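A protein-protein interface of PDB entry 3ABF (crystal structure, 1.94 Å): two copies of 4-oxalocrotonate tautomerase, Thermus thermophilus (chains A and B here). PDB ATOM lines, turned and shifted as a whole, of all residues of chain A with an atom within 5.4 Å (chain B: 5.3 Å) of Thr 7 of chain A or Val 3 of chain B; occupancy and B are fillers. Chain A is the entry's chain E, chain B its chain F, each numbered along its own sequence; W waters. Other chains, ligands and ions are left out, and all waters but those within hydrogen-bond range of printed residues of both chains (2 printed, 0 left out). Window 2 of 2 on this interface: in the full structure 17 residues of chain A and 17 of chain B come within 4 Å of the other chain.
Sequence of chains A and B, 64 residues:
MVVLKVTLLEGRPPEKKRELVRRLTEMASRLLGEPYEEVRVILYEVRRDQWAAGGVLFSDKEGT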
ATOM      1  N   LYS A   5      -3.072  28.524  20.289  1.00  0.00           N
ATOM      2  CA  LYS A   5      -1.705  28.285  19.860  1.00  0.00           C
ATOM      3  C   LYS A   5      -1.424  26.811  20.086  1.00  0.00           C
ATOM      4  O   LYS A   5      -1.617  26.292  21.189  1.00  0.00           O
ATOM      5  CB  LYS A   5      -0.741  29.132  20.682  1.00  0.00           C
ATOM      6  CG  LYS A   5       0.739  28.944  20.350  1.00  0.00           C
ATOM      7  CD  LYS A   5       1.561  29.709  21.400  1.00  0.00           C
ATOM      8  CE  LYS A   5       3.045  29.750  21.115  1.00  0.00           C
ATOM      9  NZ  LYS A   5       3.703  30.664  22.110  1.00  0.00           N
ATOM     10  N   VAL A   6      -0.975  26.133  19.039  1.00  0.00           N
ATOM     11  CA  VAL A   6      -0.677  24.721  19.157  1.00  0.00           C
ATOM     12  C   VAL A   6       0.834  24.531  19.063  1.00  0.00           C
ATOM     13  O   VAL A   6       1.446  24.851  18.040  1.00  0.00           O
ATOM     14  CB  VAL A   6      -1.340  23.914  18.018  1.00  0.00           C
ATOM     15  CG1 VAL A   6      -1.089  22.433  18.234  1.00  0.00           C
ATOM     16  CG2 VAL A   6      -2.850  24.212  17.958  1.00  0.00           C
ATOM     17  N   THR A   7       1.435  24.031  20.135  1.00  0.00           N
ATOM     18  CA  THR A   7       2.866  23.768  20.146  1.00  0.00           C
ATOM     19  C   THR A   7       3.020  22.279  19.886  1.00  0.00           C
ATOM     20  O   THR A   7       2.485  21.439  20.623  1.00  0.00           O
ATOM     21  CB  THR A   7       3.494  24.141  21.502  1.00  0.00           C
ATOM     22  OG1 THR A   7       3.363  25.555  21.692  1.00  0.00           O
ATOM     23  CG2 THR A   7       4.992  23.767  21.538  1.00  0.00           C
ATOM     24  N   LEU A   8       3.736  21.954  18.818  1.00  0.00           N
ATOM     25  CA  LEU A   8       3.939  20.565  18.428  1.00  0.00           C
ATOM     26  C   LEU A   8       5.198  20.437  17.568  1.00  0.00           C
ATOM     27  O   LEU A   8       5.615  21.393  16.917  1.00  0.00           O
ATOM     28  CB  LEU A   8       2.739  20.090  17.608  1.00  0.00           C
ATOM     29  CG  LEU A   8       2.646  20.601  16.158  1.00  0.00           C
ATOM     30  CD1 LEU A   8       1.410  20.022  15.510  1.00  0.00           C
ATOM     31  CD2 LEU A   8       2.609  22.129  16.103  1.00  0.00           C
ATOM     32  N   LEU A   9       5.787  19.250  17.555  1.00  0.00           N
ATOM     33  CA  LEU A   9       6.976  19.007  16.734  1.00  0.00           C
ATOM     34  C   LEU A   9       6.662  19.246  15.266  1.00  0.00           C
ATOM     35  O   LEU A   9       5.555  18.968  14.808  1.00  0.00           O
ATOM     36  CB  LEU A   9       7.460  17.565  16.905  1.00  0.00           C
ATOM     37  CG  LEU A   9       8.470  17.354  18.030  1.00  0.00           C
ATOM     38  CD1 LEU A   9       8.704  15.861  18.246  1.00  0.00           C
ATOM     39  CD2 LEU A   9       9.773  18.051  17.663  1.00  0.00           C
ATOM     40  N   TYR A  44       2.793  26.631  16.291  1.00  0.00           N
ATOM     41  CA  TYR A  44       4.153  26.814  16.730  1.00  0.00           C
ATOM     42  C   TYR A  44       4.837  25.461  16.578  1.00  0.00           C
ATOM     43  O   TYR A  44       4.774  24.604  17.463  1.00  0.00           O
ATOM     44  CB  TYR A  44       4.183  27.258  18.190  1.00  0.00           C
ATOM     45  CG  TYR A  44       5.573  27.383  18.755  1.00  0.00           C
ATOM     46  CD1 TYR A  44       5.841  26.970  20.057  1.00  0.00           C
ATOM     47  CD2 TYR A  44       6.619  27.920  18.000  1.00  0.00           C
ATOM     48  CE1 TYR A  44       7.107  27.086  20.603  1.00  0.00           C
ATOM     49  CE2 TYR A  44       7.913  28.044  18.546  1.00  0.00           C
ATOM     50  CZ  TYR A  44       8.139  27.623  19.851  1.00  0.00           C
ATOM     51  OH  TYR A  44       9.380  27.736  20.434  1.00  0.00           O
ATOM     52  N   VAL A  46       7.937  23.177  16.562  1.00  0.00           N
ATOM     53  CA  VAL A  46       9.264  23.155  17.146  1.00  0.00           C
ATOM     54  C   VAL A  46      10.136  22.123  16.432  1.00  0.00           C
ATOM     55  O   VAL A  46       9.671  21.058  16.053  1.00  0.00           O
ATOM     56  CB  VAL A  46       9.185  22.799  18.662  1.00  0.00           C
ATOM     57  CG1 VAL A  46      10.542  22.979  19.315  1.00  0.00           C
ATOM     58  CG2 VAL A  46       8.153  23.689  19.350  1.00  0.00           C
ATOM     59  N   TRP A  51      13.564  20.617  21.072  1.00  0.00           N
ATOM     60  CA  TRP A  51      12.534  20.020  21.917  1.00  0.00           C
ATOM     61  C   TRP A  51      13.129  18.882  22.719  1.00  0.00           C
ATOM     62  O   TRP A  51      13.642  17.925  22.143  1.00  0.00           O
ATOM     63  CB  TRP A  51      11.434  19.517  20.978  1.00  0.00           C
ATOM     64  CG  TRP A  51      10.312  18.713  21.539  1.00  0.00           C
ATOM     65  CD1 TRP A  51      10.335  17.386  21.881  1.00  0.00           C
ATOM     66  CD2 TRP A  51       8.953  19.141  21.691  1.00  0.00           C
ATOM     67  NE1 TRP A  51       9.070  16.963  22.223  1.00  0.00           N
ATOM     68  CE2 TRP A  51       8.205  18.021  22.117  1.00  0.00           C
ATOM     69  CE3 TRP A  51       8.294  20.360  21.505  1.00  0.00           C
ATOM     70  CZ2 TRP A  51       6.828  18.086  22.359  1.00  0.00           C
ATOM     71  CZ3 TRP A  51       6.921  20.425  21.744  1.00  0.00           C
ATOM     72  CH2 TRP A  51       6.206  19.294  22.166  1.00  0.00           C
ATOM     73  N   MET B   1       4.029  14.738  22.984  1.00  0.00           N
ATOM     74  CA  MET B   1       3.257  15.793  23.707  1.00  0.00           C
ATOM     75  C   MET B   1       2.847  16.923  22.773  1.00  0.00           C
ATOM     76  O   MET B   1       3.582  17.281  21.857  1.00  0.00           O
ATOM     77  CB  MET B   1       4.084  16.377  24.855  1.00  0.00           C
ATOM     78  CG  MET B   1       3.387  17.512  25.620  1.00  0.00           C
ATOM     79  SD  MET B   1       4.426  18.314  26.879  1.00  0.00           S
ATOM     80  CE  MET B   1       5.354  19.523  25.898  1.00  0.00           C
ATOM     81  N   VAL B   2       1.652  17.455  23.003  1.00  0.00           N
ATOM     82  CA  VAL B   2       1.136  18.576  22.234  1.00  0.00           C
ATOM     83  C   VAL B   2       0.546  19.517  23.268  1.00  0.00           C
ATOM     84  O   VAL B   2      -0.130  19.082  24.204  1.00  0.00           O
ATOM     85  CB  VAL B   2       0.045  18.161  21.250  1.00  0.00           C
ATOM     86  CG1 VAL B   2      -0.562  19.397  20.595  1.00  0.00           C
ATOM     87  CG2 VAL B   2       0.647  17.279  20.166  1.00  0.00           C
ATOM     88  N   VAL B   3       0.832  20.802  23.124  1.00  0.00           N
ATOM     89  CA  VAL B   3       0.321  21.768  24.073  1.00  0.00           C
ATOM     90  C   VAL B   3      -0.575  22.771  23.390  1.00  0.00           C
ATOM     91  O   VAL B   3      -0.163  23.453  22.457  1.00  0.00           O
ATOM     92  CB  VAL B   3       1.458  22.535  24.770  1.00  0.00           C
ATOM     93  CG1 VAL B   3       0.865  23.500  25.801  1.00  0.00           C
ATOM     94  CG2 VAL B   3       2.421  21.563  25.437  1.00  0.00           C
ATOM     95  N   LEU B   4      -1.819  22.846  23.845  1.00  0.00           N
ATOM     96  CA  LEU B   4      -2.755  23.793  23.284  1.00  0.00           C
ATOM     97  C   LEU B   4      -2.911  24.900  24.302  1.00  0.00           C
ATOM     98  O   LEU B   4      -3.306  24.659  25.441  1.00  0.00           O
ATOM     99  CB  LEU B   4      -4.100  23.135  23.030  1.00  0.00           C
ATOM    100  CG  LEU B   4      -4.044  21.928  22.089  1.00  0.00           C
ATOM    101  CD1 LEU B   4      -5.051  20.877  22.538  1.00  0.00           C
ATOM    102  CD2 LEU B   4      -4.337  22.387  20.674  1.00  0.00           C
ATOM    103  N   LYS B   5      -2.574  26.112  23.894  1.00  0.00           N
ATOM    104  CA  LYS B   5      -2.687  27.261  24.771  1.00  0.00           C
ATOM    105  C   LYS B   5      -3.816  28.094  24.199  1.00  0.00           C
ATOM    106  O   LYS B   5      -3.800  28.479  23.032  1.00  0.00           O
ATOM    107  CB  LYS B   5      -1.383  28.059  24.759  1.00  0.00           C
ATOM    108  CG  LYS B   5      -1.350  29.268  25.686  1.00  0.00           C
ATOM    109  CD  LYS B   5      -0.084  30.056  25.368  1.00  0.00           C
ATOM    110  CE  LYS B   5       0.076  31.286  26.201  1.00  0.00           C
ATOM    111  NZ  LYS B   5       1.341  31.953  25.790  1.00  0.00           N
ATOM    112  N   ARG B  40      -1.884  18.430  26.615  1.00  0.00           N
ATOM    113  CA  ARG B  40      -1.994  19.379  27.703  1.00  0.00           C
ATOM    114  C   ARG B  40      -2.653  20.633  27.184  1.00  0.00           C
ATOM    115  O   ARG B  40      -2.418  21.056  26.052  1.00  0.00           O
ATOM    116  CB  ARG B  40      -0.611  19.725  28.242  1.00  0.00           C
ATOM    117  CG  ARG B  40       0.340  18.531  28.326  1.00  0.00           C
ATOM    118  CD  ARG B  40       0.138  17.702  29.585  1.00  0.00           C
ATOM    119  NE  ARG B  40       0.140  18.544  30.776  1.00  0.00           N
ATOM    120  CZ  ARG B  40       0.467  18.130  31.994  1.00  0.00           C
ATOM    121  NH1 ARG B  40       0.836  16.871  32.198  1.00  0.00           N
ATOM    122  NH2 ARG B  40       0.411  18.976  33.013  1.00  0.00           N
ATOM    123  N   ILE B  42      -3.583  24.682  28.327  1.00  0.00           N
ATOM    124  CA  ILE B  42      -3.311  25.767  29.258  1.00  0.00           C
ATOM    125  C   ILE B  42      -4.264  26.891  28.892  1.00  0.00           C
ATOM    126  O   ILE B  42      -4.353  27.282  27.730  1.00  0.00           O
ATOM    127  CB  ILE B  42      -1.857  26.281  29.121  1.00  0.00           C
ATOM    128  CG1 ILE B  42      -0.878  25.190  29.585  1.00  0.00           C
ATOM    129  CG2 ILE B  42      -1.667  27.567  29.961  1.00  0.00           C
ATOM    130  CD1 ILE B  42       0.592  25.580  29.441  1.00  0.00           C
HETATM  131  O   HOH W   1       4.383  17.017  19.200  1.00  0.00           O
HETATM  132  O   HOH W   2       1.051  26.206  22.771  1.00  0.00           O
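N of Lys 5 of chain A lies within hydrogen-bond range of O of Lys 5 of chain B (2.8 Å). The backbone NH (N) of Thr 7 of chain A sits at hydrogen-bond distance from the backbone carbonyl oxygen (O) of Val 3 of chain B, at 2.9 Å. The backbone carbonyl oxygen of Lys 5 of chain A sits close to the backbone carbonyl oxygen of Val 3 of chain B (3.4 Å).
The backbone carbonyl oxygen (O) of Val 6 of chain A is in hydrogen-bond range of the backbone NH (N) of Tyr 44 of chain A (2.8 Å). The backbone carbonyl oxygen (O) of Leu 4 of chain B sits at hydrogen-bond distance from the backbone NH (N) of Ile 42 of chain B (2.9 Å). The backbone NH of Arg 40 of chain B sits at hydrogen-bond distance from the backbone carbonyl oxygen of Val 2 of chain B (3.1 Å). The backbone carbonyl oxygen (O) of Arg 40 of chain B lies within hydrogen-bond range of the backbone NH (N) of Leu 4 of chain B, 2.9 Å away.
Among the printed residues, merely in contact across the chains: Lys 5 of chain A with Leu 4 of chain B (3.5 Å), Val 6 of chain A with Val 2 of chain B (3.9 Å), Val 6 of chain A with Val 3 of chain B (3.6 Å), Val 6 of chain A with Leu 4 of chain B (3.6 Å), Thr 7 of chain A with Val 2 of chain B (3.6 Å) and Trp 51 of chain A with Met 1 of chain B (3.3 Å).
Of the printed residues of chain A, Val 3 of chain B touches Lys 5, Val 6 and Thr 7. Of the printed residues of chain A, Lys 5 of chain B touches Lys 5 (2.8 Å). Of the printed residues of chain B, Val 6 of chain A touches Val 2 (3.9 Å), Val 3 (3.6 Å) and Leu 4 (3.6 Å). Of the printed residues of chain B, Trp 51 of chain A touches Met 1 (3.3 Å). Tyr 44 of chain A touches none of the printed residues of chain B. Val 46 of chain A touches none of the printed residues of chain B. The nearest printed residue of chain B that does not touch Trp 51 of chain A is Val 2 of chain B (5.0 Å).
Of the 7 printed residues of chain B, 5 touch a printed residue of chain A. Printed residues of chain B that touch a printed residue of chain A: Met 1, Val 2, Val 3, Leu 4 and Lys 5. Among the printed residues, no Asp or Glu carboxylate lies within 4 Å of a Lys or Arg side-chain nitrogen of the other chain.
Lys 5 of chain B touches its own counterpart, Lys 5 of chain A. Of the 9 pairs that touch across the chains among the printed residues, 1 has its exchanged pair printed and touching as well.
Water W2 lies within hydrogen-bond range of OG1 of Thr 7 of chain A, O of Val 3 of chain B and O of Lys 5 of chain A. Water W1 lies within hydrogen-bond range of O of Met 1 of chain B (2.8 Å) and N of Leu 9 of chain A (3.1 Å).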
